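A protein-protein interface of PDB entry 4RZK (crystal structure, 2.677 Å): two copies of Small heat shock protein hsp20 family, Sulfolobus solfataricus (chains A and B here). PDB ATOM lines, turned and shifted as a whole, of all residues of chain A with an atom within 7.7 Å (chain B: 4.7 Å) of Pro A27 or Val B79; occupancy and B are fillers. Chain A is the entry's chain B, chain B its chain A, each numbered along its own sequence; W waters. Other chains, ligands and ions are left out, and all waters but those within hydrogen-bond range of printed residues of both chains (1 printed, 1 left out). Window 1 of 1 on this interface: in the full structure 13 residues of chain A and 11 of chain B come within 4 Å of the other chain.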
ATOM      1  N   ARG A   7       3.292   0.076  20.164  1.00  0.00           N
ATOM      2  CA  ARG A   7       3.904  -1.212  20.315  1.00  0.00           C
ATOM      3  C   ARG A   7       3.144  -1.955  21.355  1.00  0.00           C
ATOM      4  O   ARG A   7       2.474  -1.358  22.166  1.00  0.00           O
ATOM      5  CB  ARG A   7       5.330  -1.056  20.793  1.00  0.00           C
ATOM      6  CG  ARG A   7       6.152  -0.064  20.010  1.00  0.00           C
ATOM      7  CD  ARG A   7       7.493  -0.673  19.679  1.00  0.00           C
ATOM      8  NE  ARG A   7       8.582   0.285  19.728  1.00  0.00           N
ATOM      9  CZ  ARG A   7       9.468   0.344  20.703  1.00  0.00           C
ATOM     10  NH1 ARG A   7       9.389  -0.486  21.720  1.00  0.00           N
ATOM     11  NH2 ARG A   7      10.430   1.235  20.663  1.00  0.00           N
ATOM     12  N   PRO A   9       3.796  -4.024  24.500  1.00  0.00           N
ATOM     13  CA  PRO A   9       4.890  -4.229  25.436  1.00  0.00           C
ATOM     14  C   PRO A   9       4.976  -5.647  25.941  1.00  0.00           C
ATOM     15  O   PRO A   9       3.993  -6.371  25.893  1.00  0.00           O
ATOM     16  CB  PRO A   9       4.533  -3.293  26.586  1.00  0.00           C
ATOM     17  CG  PRO A   9       3.080  -3.088  26.469  1.00  0.00           C
ATOM     18  CD  PRO A   9       2.829  -3.052  25.008  1.00  0.00           C
ATOM     19  N   LEU A  10       6.151  -6.036  26.413  1.00  0.00           N
ATOM     20  CA  LEU A  10       6.309  -7.326  27.042  1.00  0.00           C
ATOM     21  C   LEU A  10       5.736  -7.270  28.434  1.00  0.00           C
ATOM     22  O   LEU A  10       6.100  -6.419  29.220  1.00  0.00           O
ATOM     23  CB  LEU A  10       7.783  -7.692  27.123  1.00  0.00           C
ATOM     24  CG  LEU A  10       8.486  -7.996  25.806  1.00  0.00           C
ATOM     25  CD1 LEU A  10       9.942  -8.315  26.052  1.00  0.00           C
ATOM     26  CD2 LEU A  10       7.822  -9.143  25.078  1.00  0.00           C
ATOM     27  N   ALA A  24       5.235  -5.052  33.212  1.00  0.00           N
ATOM     28  CA  ALA A  24       5.373  -4.728  31.813  1.00  0.00           C
ATOM     29  C   ALA A  24       6.592  -3.905  31.591  1.00  0.00           C
ATOM     30  O   ALA A  24       6.941  -3.094  32.415  1.00  0.00           O
ATOM     31  CB  ALA A  24       4.136  -4.002  31.307  1.00  0.00           C
ATOM     32  N   GLU A  25       7.229  -4.105  30.454  1.00  0.00           N
ATOM     33  CA  GLU A  25       8.353  -3.290  30.093  1.00  0.00           C
ATOM     34  C   GLU A  25       7.850  -2.243  29.143  1.00  0.00           C
ATOM     35  O   GLU A  25       7.435  -2.547  28.048  1.00  0.00           O
ATOM     36  CB  GLU A  25       9.419  -4.144  29.430  1.00  0.00           C
ATOM     37  CG  GLU A  25       9.897  -5.277  30.310  1.00  0.00           C
ATOM     38  CD  GLU A  25      10.939  -6.131  29.647  1.00  0.00           C
ATOM     39  OE1 GLU A  25      11.086  -6.020  28.431  1.00  0.00           O
ATOM     40  OE2 GLU A  25      11.609  -6.904  30.341  1.00  0.00           O
ATOM     41  N   VAL A  26       7.895  -1.000  29.592  1.00  0.00           N
ATOM     42  CA  VAL A  26       7.468   0.129  28.812  1.00  0.00           C
ATOM     43  C   VAL A  26       8.528   1.179  28.900  1.00  0.00           C
ATOM     44  O   VAL A  26       8.324   2.220  29.468  1.00  0.00           O
ATOM     45  CB  VAL A  26       6.184   0.751  29.364  1.00  0.00           C
ATOM     46  CG1 VAL A  26       4.976   0.095  28.751  1.00  0.00           C
ATOM     47  CG2 VAL A  26       6.127   0.617  30.865  1.00  0.00           C
ATOM     48  N   PRO A  27       9.664   0.916  28.304  1.00  0.00           N
ATOM     49  CA  PRO A  27      10.734   1.893  28.305  1.00  0.00           C
ATOM     50  C   PRO A  27      10.341   3.062  27.432  1.00  0.00           C
ATOM     51  O   PRO A  27       9.554   2.893  26.519  1.00  0.00           O
ATOM     52  CB  PRO A  27      11.898   1.130  27.694  1.00  0.00           C
ATOM     53  CG  PRO A  27      11.309  -0.077  27.079  1.00  0.00           C
ATOM     54  CD  PRO A  27      10.139  -0.407  27.914  1.00  0.00           C
ATOM     55  N   GLY A  28      10.889   4.230  27.718  1.00  0.00           N
ATOM     56  CA  GLY A  28      10.620   5.402  26.926  1.00  0.00           C
ATOM     57  C   GLY A  28       9.412   6.220  27.285  1.00  0.00           C
ATOM     58  O   GLY A  28       9.031   7.087  26.535  1.00  0.00           O
ATOM     59  N   VAL A  29       8.792   5.945  28.414  1.00  0.00           N
ATOM     60  CA  VAL A  29       7.716   6.793  28.877  1.00  0.00           C
ATOM     61  C   VAL A  29       7.920   7.159  30.321  1.00  0.00           C
ATOM     62  O   VAL A  29       8.503   6.403  31.063  1.00  0.00           O
ATOM     63  CB  VAL A  29       6.352   6.108  28.757  1.00  0.00           C
ATOM     64  CG1 VAL A  29       5.975   5.920  27.309  1.00  0.00           C
ATOM     65  CG2 VAL A  29       6.346   4.794  29.500  1.00  0.00           C
ATOM     66  N   ASN A  30       7.449   8.325  30.715  1.00  0.00           N
ATOM     67  CA  ASN A  30       7.402   8.721  32.107  1.00  0.00           C
ATOM     68  C   ASN A  30       6.248   8.031  32.801  1.00  0.00           C
ATOM     69  O   ASN A  30       5.350   7.555  32.156  1.00  0.00           O
ATOM     70  CB  ASN A  30       7.267  10.233  32.234  1.00  0.00           C
ATOM     71  CG  ASN A  30       8.521  10.968  31.835  1.00  0.00           C
ATOM     72  OD1 ASN A  30       9.544  10.852  32.479  1.00  0.00           O
ATOM     73  ND2 ASN A  30       8.438  11.732  30.772  1.00  0.00           N
ATOM     74  N   ALA A  49       0.214   3.833  27.287  1.00  0.00           N
ATOM     75  CA  ALA A  49       1.238   4.825  27.572  1.00  0.00           C
ATOM     76  C   ALA A  49       1.572   5.662  26.354  1.00  0.00           C
ATOM     77  O   ALA A  49       1.827   5.134  25.297  1.00  0.00           O
ATOM     78  CB  ALA A  49       2.486   4.158  28.119  1.00  0.00           C
ATOM     79  N   SER A  51       4.091   8.979  25.180  1.00  0.00           N
ATOM     80  CA  SER A  51       5.108   9.948  25.508  1.00  0.00           C
ATOM     81  C   SER A  51       5.624  10.444  24.187  1.00  0.00           C
ATOM     82  O   SER A  51       5.296   9.879  23.165  1.00  0.00           O
ATOM     83  CB  SER A  51       6.219   9.310  26.323  1.00  0.00           C
ATOM     84  OG  SER A  51       7.273   8.919  25.493  1.00  0.00           O
ATOM     85  N   ASP A  53       8.509  10.231  22.997  1.00  0.00           N
ATOM     86  CA  ASP A  53       9.291   9.100  22.516  1.00  0.00           C
ATOM     87  C   ASP A  53       8.546   7.818  22.130  1.00  0.00           C
ATOM     88  O   ASP A  53       8.880   7.194  21.142  1.00  0.00           O
ATOM     89  CB  ASP A  53      10.396   8.772  23.512  1.00  0.00           C
ATOM     90  CG  ASP A  53      11.492   9.792  23.509  1.00  0.00           C
ATOM     91  OD1 ASP A  53      12.145   9.958  22.472  1.00  0.00           O
ATOM     92  OD2 ASP A  53      11.708  10.434  24.544  1.00  0.00           O
ATOM     93  N   ARG A  54       7.566   7.411  22.922  1.00  0.00           N
ATOM     94  CA  ARG A  54       6.981   6.088  22.764  1.00  0.00           C
ATOM     95  C   ARG A  54       5.479   6.020  22.883  1.00  0.00           C
ATOM     96  O   ARG A  54       4.866   6.838  23.530  1.00  0.00           O
ATOM     97  CB  ARG A  54       7.557   5.121  23.793  1.00  0.00           C
ATOM     98  CG  ARG A  54       9.058   5.107  23.911  1.00  0.00           C
ATOM     99  CD  ARG A  54       9.693   4.175  22.910  1.00  0.00           C
ATOM    100  NE  ARG A  54      10.818   4.838  22.279  1.00  0.00           N
ATOM    101  CZ  ARG A  54      11.997   4.280  22.087  1.00  0.00           C
ATOM    102  NH1 ARG A  54      12.966   4.956  21.511  1.00  0.00           N
ATOM    103  NH2 ARG A  54      12.199   3.042  22.477  1.00  0.00           N
ATOM    104  N   GLN A  55       4.898   5.020  22.243  1.00  0.00           N
ATOM    105  CA  GLN A  55       3.502   4.686  22.417  1.00  0.00           C
ATOM    106  C   GLN A  55       3.349   3.203  22.715  1.00  0.00           C
ATOM    107  O   GLN A  55       3.913   2.389  22.021  1.00  0.00           O
ATOM    108  CB  GLN A  55       2.723   5.052  21.167  1.00  0.00           C
ATOM    109  CG  GLN A  55       1.278   5.379  21.426  1.00  0.00           C
ATOM    110  CD  GLN A  55       0.602   6.048  20.258  1.00  0.00           C
ATOM    111  OE1 GLN A  55       1.199   6.269  19.217  1.00  0.00           O
ATOM    112  NE2 GLN A  55      -0.656   6.378  20.432  1.00  0.00           N
ATOM    113  N   TYR A  56       2.576   2.860  23.737  1.00  0.00           N
ATOM    114  CA  TYR A  56       2.316   1.466  24.086  1.00  0.00           C
ATOM    115  C   TYR A  56       0.837   1.206  24.348  1.00  0.00           C
ATOM    116  O   TYR A  56       0.131   2.057  24.877  1.00  0.00           O
ATOM    117  CB  TYR A  56       3.094   1.062  25.346  1.00  0.00           C
ATOM    118  CG  TYR A  56       4.611   1.080  25.274  1.00  0.00           C
ATOM    119  CD1 TYR A  56       5.317  -0.024  24.824  1.00  0.00           C
ATOM    120  CD2 TYR A  56       5.334   2.184  25.702  1.00  0.00           C
ATOM    121  CE1 TYR A  56       6.706  -0.029  24.781  1.00  0.00           C
ATOM    122  CE2 TYR A  56       6.729   2.181  25.676  1.00  0.00           C
ATOM    123  CZ  TYR A  56       7.404   1.069  25.207  1.00  0.00           C
ATOM    124  OH  TYR A  56       8.779   1.057  25.162  1.00  0.00           O
ATOM    125  N   PHE A  75       6.952   2.100  38.946  1.00  0.00           N
ATOM    126  CA  PHE A  75       7.670   2.283  37.691  1.00  0.00           C
ATOM    127  C   PHE A  75       9.157   2.529  37.910  1.00  0.00           C
ATOM    128  O   PHE A  75       9.542   3.543  38.448  1.00  0.00           O
ATOM    129  CB  PHE A  75       7.064   3.460  36.943  1.00  0.00           C
ATOM    130  CG  PHE A  75       7.417   3.508  35.496  1.00  0.00           C
ATOM    131  CD1 PHE A  75       7.346   2.380  34.724  1.00  0.00           C
ATOM    132  CD2 PHE A  75       7.810   4.686  34.913  1.00  0.00           C
ATOM    133  CE1 PHE A  75       7.662   2.423  33.393  1.00  0.00           C
ATOM    134  CE2 PHE A  75       8.130   4.736  33.585  1.00  0.00           C
ATOM    135  CZ  PHE A  75       8.053   3.602  32.824  1.00  0.00           C
ATOM    136  N   ASN A  77      12.988   2.364  35.886  1.00  0.00           N
ATOM    137  CA  ASN A  77      13.842   2.077  34.759  1.00  0.00           C
ATOM    138  C   ASN A  77      13.044   1.476  33.627  1.00  0.00           C
ATOM    139  O   ASN A  77      13.487   0.539  32.999  1.00  0.00           O
ATOM    140  CB  ASN A  77      14.972   1.137  35.145  1.00  0.00           C
ATOM    141  CG  ASN A  77      15.933   1.750  36.121  1.00  0.00           C
ATOM    142  OD1 ASN A  77      16.179   1.196  37.173  1.00  0.00           O
ATOM    143  ND2 ASN A  77      16.490   2.884  35.772  1.00  0.00           N
ATOM    144  N   GLY A  78      11.862   2.007  33.372  1.00  0.00           N
ATOM    145  CA  GLY A  78      11.075   1.580  32.239  1.00  0.00           C
ATOM    146  C   GLY A  78      10.283   0.315  32.423  1.00  0.00           C
ATOM    147  O   GLY A  78       9.691  -0.194  31.493  1.00  0.00           O
ATOM    148  N   VAL A  79      10.270  -0.200  33.634  1.00  0.00           N
ATOM    149  CA  VAL A  79       9.517  -1.402  33.904  1.00  0.00           C
ATOM    150  C   VAL A  79       8.432  -1.103  34.905  1.00  0.00           C
ATOM    151  O   VAL A  79       8.685  -0.498  35.922  1.00  0.00           O
ATOM    152  CB  VAL A  79      10.418  -2.515  34.431  1.00  0.00           C
ATOM    153  CG1 VAL A  79      11.639  -1.914  35.082  1.00  0.00           C
ATOM    154  CG2 VAL A  79       9.661  -3.390  35.407  1.00  0.00           C
ATOM    155  N   LEU A  80       7.220  -1.541  34.607  1.00  0.00           N
ATOM    156  CA  LEU A  80       6.069  -1.192  35.411  1.00  0.00           C
ATOM    157  C   LEU A  80       5.571  -2.370  36.200  1.00  0.00           C
ATOM    158  O   LEU A  80       5.276  -3.408  35.650  1.00  0.00           O
ATOM    159  CB  LEU A  80       4.957  -0.682  34.506  1.00  0.00           C
ATOM    160  CG  LEU A  80       3.596  -0.357  35.104  1.00  0.00           C
ATOM    161  CD1 LEU A  80       3.722   0.806  36.057  1.00  0.00           C
ATOM    162  CD2 LEU A  80       2.621  -0.021  33.996  1.00  0.00           C
ATOM    163  N   VAL B  23      20.716   3.966  19.895  1.00  0.00           N
ATOM    164  CA  VAL B  23      19.679   3.905  20.905  1.00  0.00           C
ATOM    165  C   VAL B  23      19.398   2.477  21.327  1.00  0.00           C
ATOM    166  O   VAL B  23      19.174   1.626  20.497  1.00  0.00           O
ATOM    167  CB  VAL B  23      18.380   4.513  20.385  1.00  0.00           C
ATOM    168  CG1 VAL B  23      17.237   4.191  21.315  1.00  0.00           C
ATOM    169  CG2 VAL B  23      18.529   6.006  20.225  1.00  0.00           C
ATOM    170  N   ALA B  24      19.420   2.230  22.629  1.00  0.00           N
ATOM    171  CA  ALA B  24      19.179   0.908  23.168  1.00  0.00           C
ATOM    172  C   ALA B  24      18.170   0.891  24.291  1.00  0.00           C
ATOM    173  O   ALA B  24      18.233   1.703  25.187  1.00  0.00           O
ATOM    174  CB  ALA B  24      20.490   0.299  23.642  1.00  0.00           C
ATOM    175  N   GLU B  25      17.279  -0.081  24.263  1.00  0.00           N
ATOM    176  CA  GLU B  25      16.349  -0.239  25.341  1.00  0.00           C
ATOM    177  C   GLU B  25      16.826  -1.326  26.233  1.00  0.00           C
ATOM    178  O   GLU B  25      16.951  -2.463  25.835  1.00  0.00           O
ATOM    179  CB  GLU B  25      15.028  -0.675  24.811  1.00  0.00           C
ATOM    180  CG  GLU B  25      14.441   0.253  23.809  1.00  0.00           C
ATOM    181  CD  GLU B  25      13.000  -0.056  23.637  1.00  0.00           C
ATOM    182  OE1 GLU B  25      12.553  -1.090  24.139  1.00  0.00           O
ATOM    183  OE2 GLU B  25      12.295   0.747  23.017  1.00  0.00           O
ATOM    184  N   PRO B  27      15.463  -1.935  29.766  1.00  0.00           N
ATOM    185  CA  PRO B  27      14.747  -1.630  31.001  1.00  0.00           C
ATOM    186  C   PRO B  27      14.966  -2.677  32.094  1.00  0.00           C
ATOM    187  O   PRO B  27      15.186  -3.852  31.804  1.00  0.00           O
ATOM    188  CB  PRO B  27      13.291  -1.593  30.554  1.00  0.00           C
ATOM    189  CG  PRO B  27      13.239  -2.500  29.384  1.00  0.00           C
ATOM    190  CD  PRO B  27      14.554  -2.377  28.692  1.00  0.00           C
ATOM    191  N   ASN B  74      23.316   9.182  27.510  1.00  0.00           N
ATOM    192  CA  ASN B  74      22.234   9.496  28.421  1.00  0.00           C
ATOM    193  C   ASN B  74      21.264   8.347  28.618  1.00  0.00           C
ATOM    194  O   ASN B  74      21.024   7.582  27.711  1.00  0.00           O
ATOM    195  CB  ASN B  74      21.497  10.733  27.938  1.00  0.00           C
ATOM    196  CG  ASN B  74      20.856  11.501  29.067  1.00  0.00           C
ATOM    197  OD1 ASN B  74      21.535  12.117  29.878  1.00  0.00           O
ATOM    198  ND2 ASN B  74      19.537  11.469  29.123  1.00  0.00           N
ATOM    199  N   PHE B  75      20.700   8.244  29.811  1.00  0.00           N
ATOM    200  CA  PHE B  75      19.770   7.180  30.135  1.00  0.00           C
ATOM    201  C   PHE B  75      18.459   7.794  30.579  1.00  0.00           C
ATOM    202  O   PHE B  75      18.456   8.680  31.400  1.00  0.00           O
ATOM    203  CB  PHE B  75      20.354   6.340  31.262  1.00  0.00           C
ATOM    204  CG  PHE B  75      19.691   5.019  31.453  1.00  0.00           C
ATOM    205  CD1 PHE B  75      19.320   4.256  30.381  1.00  0.00           C
ATOM    206  CD2 PHE B  75      19.459   4.540  32.711  1.00  0.00           C
ATOM    207  CE1 PHE B  75      18.718   3.038  30.560  1.00  0.00           C
ATOM    208  CE2 PHE B  75      18.861   3.324  32.898  1.00  0.00           C
ATOM    209  CZ  PHE B  75      18.490   2.572  31.823  1.00  0.00           C
ATOM    210  N   LYS B  76      17.347   7.369  30.009  1.00  0.00           N
ATOM    211  CA  LYS B  76      16.058   7.842  30.479  1.00  0.00           C
ATOM    212  C   LYS B  76      15.003   6.766  30.458  1.00  0.00           C
ATOM    213  O   LYS B  76      14.710   6.219  29.423  1.00  0.00           O
ATOM    214  CB  LYS B  76      15.589   9.008  29.625  1.00  0.00           C
ATOM    215  CG  LYS B  76      14.440   9.792  30.211  1.00  0.00           C
ATOM    216  CD  LYS B  76      14.239  11.087  29.463  1.00  0.00           C
ATOM    217  CE  LYS B  76      12.924  11.724  29.844  1.00  0.00           C
ATOM    218  NZ  LYS B  76      12.223  12.289  28.669  1.00  0.00           N
ATOM    219  N   ASN B  77      14.394   6.489  31.591  1.00  0.00           N
ATOM    220  CA  ASN B  77      13.254   5.601  31.607  1.00  0.00           C
ATOM    221  C   ASN B  77      13.527   4.265  30.946  1.00  0.00           C
ATOM    222  O   ASN B  77      12.679   3.741  30.263  1.00  0.00           O
ATOM    223  CB  ASN B  77      12.057   6.267  30.956  1.00  0.00           C
ATOM    224  CG  ASN B  77      11.400   7.282  31.854  1.00  0.00           C
ATOM    225  OD1 ASN B  77      11.118   7.006  33.003  1.00  0.00           O
ATOM    226  ND2 ASN B  77      11.158   8.460  31.332  1.00  0.00           N
ATOM    227  N   GLY B  78      14.703   3.708  31.173  1.00  0.00           N
ATOM    228  CA  GLY B  78      15.069   2.431  30.601  1.00  0.00           C
ATOM    229  C   GLY B  78      15.627   2.469  29.200  1.00  0.00           C
ATOM    230  O   GLY B  78      15.874   1.440  28.614  1.00  0.00           O
ATOM    231  N   VAL B  79      15.831   3.653  28.654  1.00  0.00           N
ATOM    232  CA  VAL B  79      16.350   3.756  27.302  1.00  0.00           C
ATOM    233  C   VAL B  79      17.707   4.418  27.242  1.00  0.00           C
ATOM    234  O   VAL B  79      17.910   5.472  27.792  1.00  0.00           O
ATOM    235  CB  VAL B  79      15.388   4.500  26.379  1.00  0.00           C
ATOM    236  CG1 VAL B  79      16.085   4.875  25.093  1.00  0.00           C
ATOM    237  CG2 VAL B  79      14.187   3.636  26.082  1.00  0.00           C
ATOM    238  N   LEU B  80      18.637   3.785  26.552  1.00  0.00           N
ATOM    239  CA  LEU B  80      19.974   4.312  26.493  1.00  0.00           C
ATOM    240  C   LEU B  80      20.255   4.899  25.132  1.00  0.00           C
ATOM    241  O   LEU B  80      20.071   4.265  24.117  1.00  0.00           O
ATOM    242  CB  LEU B  80      20.989   3.233  26.836  1.00  0.00           C
ATOM    243  CG  LEU B  80      22.447   3.657  26.916  1.00  0.00           C
ATOM    244  CD1 LEU B  80      22.811   4.101  28.314  1.00  0.00           C
ATOM    245  CD2 LEU B  80      23.333   2.507  26.496  1.00  0.00           C
ATOM    246  N   GLU B  81      20.688   6.145  25.143  1.00  0.00           N
ATOM    247  CA  GLU B  81      21.018   6.871  23.950  1.00  0.00           C
ATOM    248  C   GLU B  81      22.457   7.287  24.077  1.00  0.00           C
ATOM    249  O   GLU B  81      22.830   7.931  25.036  1.00  0.00           O
ATOM    250  CB  GLU B  81      20.157   8.116  23.882  1.00  0.00           C
ATOM    251  CG  GLU B  81      19.739   8.533  22.494  1.00  0.00           C
ATOM    252  CD  GLU B  81      18.823   9.731  22.514  1.00  0.00           C
ATOM    253  OE1 GLU B  81      19.315  10.844  22.735  1.00  0.00           O
ATOM    254  OE2 GLU B  81      17.611   9.563  22.313  1.00  0.00           O
HETATM  255  O   HOH W   1      11.436   4.845  34.779  1.00  0.00           O
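The side-chain hydroxyl (OH) of Tyr A56 sits at hydrogen-bond distance from the backbone carbonyl oxygen (O) of Pro A27 (2.4 Å).
The backbone NH (N) of Val A26 sits at hydrogen-bond distance from the backbone carbonyl oxygen (O) of Gly A78, at 2.7 Å.
N of Arg A54 sits at hydrogen-bond distance from OG of Ser A51.
O of Gly A28 is in hydrogen-bond range of OG of Ser A51, at 2.7 Å.
O of Gln A55 sits at hydrogen-bond distance from N of Arg A7, 3.0 Å away.
Among the printed residues, pairs that only touch across the chains: Pro A27 with Glu B25, Pro A27 with Pro B27, Pro A27 with Asn B77, Pro A27 with Val B79, Gly A28 with Val B79, Phe A75 with Asn B77, Asn A77 with Pro B27, Asn A77 with Phe B75, Asn A77 with Asn B77, Asn A77 with Gly B78, Gly A78 with Pro B27, Gly A78 with Asn B77 and Gly A78 with Gly B78.
Water W1 lies within hydrogen-bond range of OD1 of Asn B77, N of Asn A77 and N of Gly A78.
The side-chain carboxylate (OE2) of Glu B25 lies within salt-bridge range of the guanidinium group (NH2) of Arg A7, at 3.0 Å.
O of Val A29 lies close to OD1 of Asn B77, at 3.3 Å.
The side-chain amide nitrogen (ND2) of Asn B77 is in hydrogen-bond range of the side-chain amide oxygen (OD1) of Asn A30, at 3.1 Å.
OE2 of Glu B25 sits close to NH2 of Arg A54 (2.4 Å).
The backbone NH (N) of Gly A28 is in hydrogen-bond range of the backbone carbonyl oxygen (O) of Asn B77, at 3.1 Å.
Printed residues of chain B that touch a printed residue of chain A: Glu B25, Pro B27, Phe B75, Asn B77, Gly B78 and Val B79.
Hydrophobic or aromatic side chains of chain B within 4 Å of the printed part of chain A: Pro B27, Phe B75 and Val B79.
Along chain B the printed residues that touch a printed residue of chain A span positions 25 to 79.
Printed residues of chain A that touch a printed residue of chain B: Arg A7, Pro A27, Gly A28, Val A29, Asn A30, Arg A54, Phe A75, Asn A77 and Gly A78.
Pro A9 touches none of the printed residues of chain B.
Pro A27 touches four residues of chain B.
Printed residues of chain B within 4 Å of Val A29: Asn B77.
Of the printed residues of chain B, Asn A30 touches Asn B77 (3.1 Å).
Of the printed residues of chain B, Asn A77 touches Pro B27, Phe B75, Asn B77 and Gly B78.
Of the printed residues of chain A, Glu B25 touches Arg A7, Pro A27 and Arg A54.
Printed residues of chain A within 4 Å of Phe B75: Asn A77.
Of chain A, only Asn A77 and Gly A78 come within 4 Å of Gly B78.
Val B79 touches just these residues of chain A: Pro A27 (3.8 Å) and Gly A28 (3.7 Å).
The nearest residue of chain B that does not touch Pro A27 is Gly B78 (4.1 Å).
The nearest residue of chain A that does not touch Val B79 is Arg A54 (4.2 Å).
Pro A27 touches its own counterpart, Pro B27.
Asn A77 touches Gly B78, and with the chains exchanged Gly A78 touches Asn B77.
Gly A78 touches Pro B27, but with the chains exchanged Pro A27 does not touch Gly B78 (4.1 Å).
Gly A78 touches its own counterpart, Gly B78.
Positions printed for both chains: 24, 25, 27, 75, 77, 78, 79 and 80.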
